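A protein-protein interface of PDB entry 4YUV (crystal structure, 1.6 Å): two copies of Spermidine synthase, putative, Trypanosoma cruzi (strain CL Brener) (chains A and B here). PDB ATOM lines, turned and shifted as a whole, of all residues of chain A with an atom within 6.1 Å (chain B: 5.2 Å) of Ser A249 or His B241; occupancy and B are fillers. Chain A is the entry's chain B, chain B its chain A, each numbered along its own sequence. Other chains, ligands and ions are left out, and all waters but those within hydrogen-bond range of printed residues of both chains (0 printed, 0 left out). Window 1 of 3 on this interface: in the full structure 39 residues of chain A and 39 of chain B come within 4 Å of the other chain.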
ATOM      1  N   GLU A 211       0.534 -29.669 -14.113  1.00  0.00           N
ATOM      2  CA  GLU A 211       1.276 -28.452 -14.418  1.00  0.00           C
ATOM      3  C   GLU A 211       0.485 -27.179 -14.076  1.00  0.00           C
ATOM      4  O   GLU A 211      -0.502 -27.228 -13.371  1.00  0.00           O
ATOM      5  CB  GLU A 211       1.838 -28.442 -15.889  1.00  0.00           C
ATOM      6  CG  GLU A 211       2.777 -29.633 -16.283  1.00  0.00           C
ATOM      7  CD  GLU A 211       4.115 -29.687 -15.539  1.00  0.00           C
ATOM      8  OE1 GLU A 211       4.439 -28.805 -14.688  1.00  0.00           O
ATOM      9  OE2 GLU A 211       4.864 -30.666 -15.748  1.00  0.00           O
ATOM     10  N   SER A 212       1.020 -26.043 -14.511  1.00  0.00           N
ATOM     11  CA  SER A 212       0.629 -24.693 -14.018  1.00  0.00           C
ATOM     12  C   SER A 212      -0.245 -23.964 -15.019  1.00  0.00           C
ATOM     13  O   SER A 212       0.090 -23.865 -16.245  1.00  0.00           O
ATOM     14  CB  SER A 212       1.916 -23.854 -13.741  1.00  0.00           C
ATOM     15  OG  SER A 212       1.584 -22.437 -13.614  1.00  0.00           O
ATOM     16  N   ILE A 213      -1.314 -23.359 -14.531  1.00  0.00           N
ATOM     17  CA  ILE A 213      -2.128 -22.483 -15.418  1.00  0.00           C
ATOM     18  C   ILE A 213      -1.489 -21.169 -15.811  1.00  0.00           C
ATOM     19  O   ILE A 213      -1.997 -20.459 -16.708  1.00  0.00           O
ATOM     20  CB  ILE A 213      -3.521 -22.104 -14.842  1.00  0.00           C
ATOM     21  CG1 ILE A 213      -3.343 -21.391 -13.507  1.00  0.00           C
ATOM     22  CG2 ILE A 213      -4.318 -23.396 -14.601  1.00  0.00           C
ATOM     23  CD1 ILE A 213      -4.675 -20.912 -13.014  1.00  0.00           C
ATOM     24  N   TRP A 214      -0.440 -20.800 -15.103  1.00  0.00           N
ATOM     25  CA  TRP A 214       0.241 -19.486 -15.327  1.00  0.00           C
ATOM     26  C   TRP A 214       1.377 -19.739 -16.331  1.00  0.00           C
ATOM     27  O   TRP A 214       1.724 -18.813 -17.145  1.00  0.00           O
ATOM     28  CB  TRP A 214       0.871 -19.016 -14.030  1.00  0.00           C
ATOM     29  CG  TRP A 214      -0.130 -18.599 -13.040  1.00  0.00           C
ATOM     30  CD1 TRP A 214      -0.468 -19.308 -11.883  1.00  0.00           C
ATOM     31  CD2 TRP A 214      -0.956 -17.429 -13.065  1.00  0.00           C
ATOM     32  NE1 TRP A 214      -1.419 -18.596 -11.206  1.00  0.00           N
ATOM     33  CE2 TRP A 214      -1.737 -17.449 -11.902  1.00  0.00           C
ATOM     34  CE3 TRP A 214      -1.048 -16.320 -13.933  1.00  0.00           C
ATOM     35  CZ2 TRP A 214      -2.612 -16.415 -11.559  1.00  0.00           C
ATOM     36  CZ3 TRP A 214      -1.947 -15.282 -13.608  1.00  0.00           C
ATOM     37  CH2 TRP A 214      -2.717 -15.363 -12.415  1.00  0.00           C
ATOM     38  N   TYR A 237      -9.654 -30.109 -14.650  1.00  0.00           N
ATOM     39  CA  TYR A 237      -8.407 -29.700 -13.907  1.00  0.00           C
ATOM     40  C   TYR A 237      -8.724 -29.122 -12.545  1.00  0.00           C
ATOM     41  O   TYR A 237      -9.582 -28.258 -12.405  1.00  0.00           O
ATOM     42  CB  TYR A 237      -7.804 -28.593 -14.811  1.00  0.00           C
ATOM     43  CG  TYR A 237      -6.485 -28.028 -14.314  1.00  0.00           C
ATOM     44  CD1 TYR A 237      -5.220 -28.514 -14.726  1.00  0.00           C
ATOM     45  CD2 TYR A 237      -6.519 -26.912 -13.485  1.00  0.00           C
ATOM     46  CE1 TYR A 237      -4.017 -27.948 -14.239  1.00  0.00           C
ATOM     47  CE2 TYR A 237      -5.321 -26.331 -12.996  1.00  0.00           C
ATOM     48  CZ  TYR A 237      -4.073 -26.809 -13.418  1.00  0.00           C
ATOM     49  OH  TYR A 237      -2.931 -26.160 -12.950  1.00  0.00           O
ATOM     50  N   LEU A 239      -7.093 -27.231  -9.312  1.00  0.00           N
ATOM     51  CA  LEU A 239      -5.990 -26.326  -8.969  1.00  0.00           C
ATOM     52  C   LEU A 239      -5.768 -26.390  -7.466  1.00  0.00           C
ATOM     53  O   LEU A 239      -6.759 -26.396  -6.673  1.00  0.00           O
ATOM     54  CB  LEU A 239      -6.509 -24.920  -9.368  1.00  0.00           C
ATOM     55  CG  LEU A 239      -5.662 -23.736  -9.049  1.00  0.00           C
ATOM     56  CD1 LEU A 239      -4.354 -23.791  -9.834  1.00  0.00           C
ATOM     57  CD2 LEU A 239      -6.392 -22.454  -9.496  1.00  0.00           C
ATOM     58  N   MET A 240      -4.500 -26.342  -7.093  1.00  0.00           N
ATOM     59  CA  MET A 240      -4.147 -26.352  -5.655  1.00  0.00           C
ATOM     60  C   MET A 240      -2.986 -25.433  -5.322  1.00  0.00           C
ATOM     61  O   MET A 240      -2.195 -25.099  -6.187  1.00  0.00           O
ATOM     62  CB  MET A 240      -3.808 -27.774  -5.246  1.00  0.00           C
ATOM     63  CG  MET A 240      -2.462 -28.261  -5.778  1.00  0.00           C
ATOM     64  SD  MET A 240      -2.186 -30.074  -5.840  1.00  0.00           S
ATOM     65  CE  MET A 240      -2.942 -30.413  -7.396  1.00  0.00           C
ATOM     66  N   HIS A 241      -2.922 -25.082  -4.062  1.00  0.00           N
ATOM     67  CA  HIS A 241      -1.925 -24.055  -3.510  1.00  0.00           C
ATOM     68  C   HIS A 241      -0.689 -24.734  -2.966  1.00  0.00           C
ATOM     69  O   HIS A 241      -0.746 -25.405  -1.901  1.00  0.00           O
ATOM     70  CB  HIS A 241      -2.592 -23.373  -2.365  1.00  0.00           C
ATOM     71  CG  HIS A 241      -3.624 -22.374  -2.759  1.00  0.00           C
ATOM     72  ND1 HIS A 241      -4.981 -22.644  -2.863  1.00  0.00           N
ATOM     73  CD2 HIS A 241      -3.471 -21.051  -2.996  1.00  0.00           C
ATOM     74  CE1 HIS A 241      -5.625 -21.512  -3.172  1.00  0.00           C
ATOM     75  NE2 HIS A 241      -4.715 -20.542  -3.236  1.00  0.00           N
ATOM     76  N   VAL A 242       0.404 -24.616  -3.717  1.00  0.00           N
ATOM     77  CA  VAL A 242       1.691 -25.230  -3.281  1.00  0.00           C
ATOM     78  C   VAL A 242       2.779 -24.165  -3.353  1.00  0.00           C
ATOM     79  O   VAL A 242       3.203 -23.820  -4.454  1.00  0.00           O
ATOM     80  CB  VAL A 242       2.065 -26.487  -4.076  1.00  0.00           C
ATOM     81  CG1 VAL A 242       3.379 -27.067  -3.492  1.00  0.00           C
ATOM     82  CG2 VAL A 242       0.902 -27.529  -4.172  1.00  0.00           C
ATOM     83  N   PRO A 243       3.122 -23.576  -2.185  1.00  0.00           N
ATOM     84  CA  PRO A 243       4.110 -22.461  -2.256  1.00  0.00           C
ATOM     85  C   PRO A 243       5.423 -22.724  -2.944  1.00  0.00           C
ATOM     86  O   PRO A 243       5.971 -21.789  -3.563  1.00  0.00           O
ATOM     87  CB  PRO A 243       4.374 -22.098  -0.797  1.00  0.00           C
ATOM     88  CG  PRO A 243       3.060 -22.443  -0.096  1.00  0.00           C
ATOM     89  CD  PRO A 243       2.646 -23.771  -0.806  1.00  0.00           C
ATOM     90  N   TYR A 245       6.030 -24.853  -5.528  1.00  0.00           N
ATOM     91  CA  TYR A 245       6.009 -25.138  -6.920  1.00  0.00           C
ATOM     92  C   TYR A 245       6.001 -23.837  -7.699  1.00  0.00           C
ATOM     93  O   TYR A 245       5.572 -22.794  -7.146  1.00  0.00           O
ATOM     94  CB  TYR A 245       4.837 -26.062  -7.386  1.00  0.00           C
ATOM     95  CG  TYR A 245       4.992 -27.543  -6.958  1.00  0.00           C
ATOM     96  CD1 TYR A 245       6.247 -28.173  -6.927  1.00  0.00           C
ATOM     97  CD2 TYR A 245       3.883 -28.324  -6.666  1.00  0.00           C
ATOM     98  CE1 TYR A 245       6.370 -29.523  -6.553  1.00  0.00           C
ATOM     99  CE2 TYR A 245       4.014 -29.663  -6.311  1.00  0.00           C
ATOM    100  CZ  TYR A 245       5.261 -30.255  -6.275  1.00  0.00           C
ATOM    101  OH  TYR A 245       5.277 -31.632  -5.863  1.00  0.00           O
ATOM    102  N   PRO A 246       6.434 -23.902  -8.993  1.00  0.00           N
ATOM    103  CA  PRO A 246       6.542 -22.593  -9.737  1.00  0.00           C
ATOM    104  C   PRO A 246       5.228 -21.774  -9.779  1.00  0.00           C
ATOM    105  O   PRO A 246       4.198 -22.315 -10.149  1.00  0.00           O
ATOM    106  CB  PRO A 246       6.997 -22.995 -11.139  1.00  0.00           C
ATOM    107  CG  PRO A 246       7.863 -24.230 -10.831  1.00  0.00           C
ATOM    108  CD  PRO A 246       7.200 -24.981  -9.668  1.00  0.00           C
ATOM    109  N   CYS A 247       5.301 -20.507  -9.366  1.00  0.00           N
ATOM    110  CA  CYS A 247       4.150 -19.595  -9.369  1.00  0.00           C
ATOM    111  C   CYS A 247       3.180 -19.971  -8.254  1.00  0.00           C
ATOM    112  O   CYS A 247       2.167 -19.315  -8.130  1.00  0.00           O
ATOM    113  CB  CYS A 247       3.376 -19.496 -10.693  1.00  0.00           C
ATOM    114  SG  CYS A 247       4.324 -18.644 -11.980  1.00  0.00           S
ATOM    115  N   GLY A 248       3.535 -20.946  -7.355  1.00  0.00           N
ATOM    116  CA  GLY A 248       2.792 -21.154  -6.139  1.00  0.00           C
ATOM    117  C   GLY A 248       1.531 -22.019  -6.232  1.00  0.00           C
ATOM    118  O   GLY A 248       0.648 -22.029  -5.340  1.00  0.00           O
ATOM    119  N   SER A 249       1.380 -22.662  -7.389  1.00  0.00           N
ATOM    120  CA  SER A 249       0.316 -23.623  -7.540  1.00  0.00           C
ATOM    121  C   SER A 249       0.670 -24.642  -8.555  1.00  0.00           C
ATOM    122  O   SER A 249       1.665 -24.539  -9.244  1.00  0.00           O
ATOM    123  CB  SER A 249      -0.929 -22.903  -8.037  1.00  0.00           C
ATOM    124  OG  SER A 249      -0.827 -22.333  -9.362  1.00  0.00           O
ATOM    125  N   ILE A 250      -0.171 -25.655  -8.622  1.00  0.00           N
ATOM    126  CA  ILE A 250      -0.051 -26.706  -9.659  1.00  0.00           C
ATOM    127  C   ILE A 250      -1.445 -27.318  -9.775  1.00  0.00           C
ATOM    128  O   ILE A 250      -2.344 -27.010  -8.968  1.00  0.00           O
ATOM    129  CB  ILE A 250       1.055 -27.755  -9.317  1.00  0.00           C
ATOM    130  CG1 ILE A 250       1.507 -28.569 -10.546  1.00  0.00           C
ATOM    131  CG2 ILE A 250       0.650 -28.711  -8.164  1.00  0.00           C
ATOM    132  CD1 ILE A 250       2.906 -29.217 -10.353  1.00  0.00           C
ATOM    133  N   GLY A 251      -1.641 -28.179 -10.766  1.00  0.00           N
ATOM    134  CA  GLY A 251      -2.977 -28.791 -10.884  1.00  0.00           C
ATOM    135  C   GLY A 251      -2.844 -30.253 -11.183  1.00  0.00           C
ATOM    136  O   GLY A 251      -1.743 -30.847 -11.355  1.00  0.00           O
ATOM    137  N   PRO A 294      -9.664 -19.496 -12.355  1.00  0.00           N
ATOM    138  CA  PRO A 294      -9.664 -18.114 -12.859  1.00  0.00           C
ATOM    139  C   PRO A 294     -10.259 -18.048 -14.291  1.00  0.00           C
ATOM    140  O   PRO A 294     -10.023 -18.957 -15.108  1.00  0.00           O
ATOM    141  CB  PRO A 294      -8.151 -17.839 -13.007  1.00  0.00           C
ATOM    142  CG  PRO A 294      -7.477 -18.625 -11.864  1.00  0.00           C
ATOM    143  CD  PRO A 294      -8.262 -19.934 -11.989  1.00  0.00           C
ATOM    144  N   VAL B  80      -5.576 -10.103 -10.523  1.00  0.00           N
ATOM    145  CA  VAL B  80      -6.178 -11.024  -9.531  1.00  0.00           C
ATOM    146  C   VAL B  80      -6.627 -10.330  -8.289  1.00  0.00           C
ATOM    147  O   VAL B  80      -7.815 -10.314  -7.923  1.00  0.00           O
ATOM    148  CB  VAL B  80      -5.188 -12.134  -9.132  1.00  0.00           C
ATOM    149  CG1 VAL B  80      -5.885 -13.076  -8.138  1.00  0.00           C
ATOM    150  CG2 VAL B  80      -4.744 -12.942 -10.339  1.00  0.00           C
ATOM    151  N   LEU B 239      -9.405 -16.486  -0.167  1.00  0.00           N
ATOM    152  CA  LEU B 239      -8.039 -16.837  -0.607  1.00  0.00           C
ATOM    153  C   LEU B 239      -7.962 -16.631  -2.140  1.00  0.00           C
ATOM    154  O   LEU B 239      -8.897 -17.037  -2.798  1.00  0.00           O
ATOM    155  CB  LEU B 239      -7.810 -18.323  -0.198  1.00  0.00           C
ATOM    156  CG  LEU B 239      -6.510 -18.963  -0.540  1.00  0.00           C
ATOM    157  CD1 LEU B 239      -5.275 -18.307   0.131  1.00  0.00           C
ATOM    158  CD2 LEU B 239      -6.595 -20.442  -0.067  1.00  0.00           C
ATOM    159  N   MET B 240      -6.821 -16.169  -2.609  1.00  0.00           N
ATOM    160  CA  MET B 240      -6.668 -15.979  -4.057  1.00  0.00           C
ATOM    161  C   MET B 240      -5.257 -16.363  -4.511  1.00  0.00           C
ATOM    162  O   MET B 240      -4.285 -16.286  -3.738  1.00  0.00           O
ATOM    163  CB  MET B 240      -7.046 -14.563  -4.450  1.00  0.00           C
ATOM    164  CG  MET B 240      -5.908 -13.538  -4.142  1.00  0.00           C
ATOM    165  SD  MET B 240      -6.641 -11.838  -4.033  1.00  0.00           S
ATOM    166  CE  MET B 240      -7.298 -11.808  -2.334  1.00  0.00           C
ATOM    167  N   HIS B 241      -5.151 -16.685  -5.782  1.00  0.00           N
ATOM    168  CA  HIS B 241      -3.819 -17.083  -6.359  1.00  0.00           C
ATOM    169  C   HIS B 241      -3.114 -15.923  -6.987  1.00  0.00           C
ATOM    170  O   HIS B 241      -3.575 -15.428  -8.015  1.00  0.00           O
ATOM    171  CB  HIS B 241      -4.135 -18.086  -7.483  1.00  0.00           C
ATOM    172  CG  HIS B 241      -4.545 -19.427  -7.012  1.00  0.00           C
ATOM    173  ND1 HIS B 241      -5.853 -19.841  -6.833  1.00  0.00           N
ATOM    174  CD2 HIS B 241      -3.776 -20.501  -6.792  1.00  0.00           C
ATOM    175  CE1 HIS B 241      -5.858 -21.122  -6.471  1.00  0.00           C
ATOM    176  NE2 HIS B 241      -4.622 -21.533  -6.445  1.00  0.00           N
ATOM    177  N   VAL B 242      -1.997 -15.497  -6.403  1.00  0.00           N
ATOM    178  CA  VAL B 242      -1.165 -14.405  -6.921  1.00  0.00           C
ATOM    179  C   VAL B 242       0.265 -14.914  -6.903  1.00  0.00           C
ATOM    180  O   VAL B 242       0.907 -14.989  -5.833  1.00  0.00           O
ATOM    181  CB  VAL B 242      -1.255 -13.142  -6.071  1.00  0.00           C
ATOM    182  CG1 VAL B 242      -0.531 -11.970  -6.804  1.00  0.00           C
ATOM    183  CG2 VAL B 242      -2.715 -12.755  -5.855  1.00  0.00           C
ATOM    184  N   PRO B 243       0.825 -15.232  -8.072  1.00  0.00           N
ATOM    185  CA  PRO B 243       2.181 -15.839  -8.208  1.00  0.00           C
ATOM    186  C   PRO B 243       3.291 -14.998  -7.593  1.00  0.00           C
ATOM    187  O   PRO B 243       4.226 -15.542  -6.976  1.00  0.00           O
ATOM    188  CB  PRO B 243       2.358 -15.964  -9.715  1.00  0.00           C
ATOM    189  CG  PRO B 243       1.056 -16.340 -10.138  1.00  0.00           C
ATOM    190  CD  PRO B 243       0.129 -15.354  -9.361  1.00  0.00           C
ATOM    191  N   GLY B 248       2.865 -17.316  -3.075  1.00  0.00           N
ATOM    192  CA  GLY B 248       1.901 -17.551  -4.196  1.00  0.00           C
ATOM    193  C   GLY B 248       0.416 -17.298  -3.940  1.00  0.00           C
ATOM    194  O   GLY B 248      -0.408 -17.615  -4.795  1.00  0.00           O
ATOM    195  N   SER B 249       0.088 -16.738  -2.771  1.00  0.00           N
ATOM    196  CA  SER B 249      -1.268 -16.383  -2.525  1.00  0.00           C
ATOM    197  C   SER B 249      -1.345 -15.253  -1.569  1.00  0.00           C
ATOM    198  O   SER B 249      -0.360 -14.921  -0.869  1.00  0.00           O
ATOM    199  CB  SER B 249      -2.120 -17.541  -1.964  1.00  0.00           C
ATOM    200  OG  SER B 249      -1.568 -18.069  -0.728  1.00  0.00           O
ATOM    201  N   TYR B 281      -9.970 -12.957 -13.910  1.00  0.00           N
ATOM    202  CA  TYR B 281      -9.920 -13.861 -12.772  1.00  0.00           C
ATOM    203  C   TYR B 281     -11.243 -14.122 -12.140  1.00  0.00           C
ATOM    204  O   TYR B 281     -11.761 -15.237 -12.076  1.00  0.00           O
ATOM    205  CB  TYR B 281      -8.856 -13.344 -11.740  1.00  0.00           C
ATOM    206  CG  TYR B 281      -8.597 -14.283 -10.524  1.00  0.00           C
ATOM    207  CD1 TYR B 281      -9.429 -14.238  -9.405  1.00  0.00           C
ATOM    208  CD2 TYR B 281      -7.512 -15.211 -10.558  1.00  0.00           C
ATOM    209  CE1 TYR B 281      -9.179 -15.073  -8.334  1.00  0.00           C
ATOM    210  CE2 TYR B 281      -7.260 -16.030  -9.473  1.00  0.00           C
ATOM    211  CZ  TYR B 281      -8.098 -15.954  -8.407  1.00  0.00           C
ATOM    212  OH  TYR B 281      -7.792 -16.792  -7.320  1.00  0.00           O
ATOM    213  N   MET B 286     -15.614 -18.469  -8.829  1.00  0.00           N
ATOM    214  CA  MET B 286     -14.357 -18.182  -8.140  1.00  0.00           C
ATOM    215  C   MET B 286     -14.658 -17.448  -6.790  1.00  0.00           C
ATOM    216  O   MET B 286     -13.917 -17.623  -5.760  1.00  0.00           O
ATOM    217  CB  MET B 286     -13.438 -17.295  -8.995  1.00  0.00           C
ATOM    218  CG  MET B 286     -12.744 -18.086 -10.123  1.00  0.00           C
ATOM    219  SD  MET B 286     -11.667 -19.414  -9.467  1.00  0.00           S
ATOM    220  CE  MET B 286     -10.333 -18.479  -8.916  1.00  0.00           C
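A ring nitrogen (NE2) of His B241 sits at hydrogen-bond distance from a ring nitrogen (NE2) of His A241 (3.4 Å).
N of Pro A294 lies close to SD of Met B286 (3.5 Å).
The backbone NH (N) of His B241 sits at hydrogen-bond distance from the side-chain hydroxyl (OH) of Tyr B281, at 3.1 Å.
The backbone NH of Trp A214 lies within hydrogen-bond range of the side-chain hydroxyl of Ser A212 (3.0 Å).
Among the printed residues, pairs that only touch across the chains: Trp A214 with Val B80, Trp A214 with His B241, Trp A214 with Pro B243, Leu A239 with His B241, His A241 with Leu B239, His A241 with Ser B249, Cys A247 with Pro B243, Ser A249 with His B241 and Pro A294 with Tyr B281.
Printed residues of chain B within 4 Å of Trp A214: Val B80, His B241 and Pro B243.
Tyr A245 touches none of the printed residues of chain B.
Of the printed residues of chain B, Cys A247 touches Pro B243.
Of the printed residues of chain B, Ser A249 touches His B241.
Met B240 touches none of the printed residues of chain A.
Printed residues of chain A within 4 Å of His B241: Trp A214, Leu A239, His A241 and Ser A249.
The nearest printed residue of chain B that does not touch Ser A249 is Gly B248 (5.9 Å).
The nearest residue of chain A that does not touch His B241 is Met A240 (4.3 Å).
The nearest printed residue of chain A that does not touch Ser B249 is Gly A248 (5.9 Å).
Of the 18 printed residues of chain A, 6 touch a printed residue of chain B.
Printed residues of chain A that touch a printed residue of chain B: Trp A214, Leu A239, His A241, Cys A247, Ser A249 and Pro A294.
Hydrophobic or aromatic side chains of chain A that line the printed part of chain B: Trp A214, Leu A239, His A241 and Pro A294.
Along chain A the printed residues that touch a printed residue of chain B span positions 214 to 294.
Among the printed residues, 11 pairs touch across the chains.
Among the printed residues, no Asp or Glu carboxylate lies within 4 Å of a Lys or Arg side-chain nitrogen of the other chain.
Leu A239 touches His B241, and with the chains exchanged His A241 touches Leu B239.
His B241 touches its own counterpart, His A241.
His A241 touches Ser B249, and with the chains exchanged Ser A249 touches His B241.
7 positions are printed for both chains.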
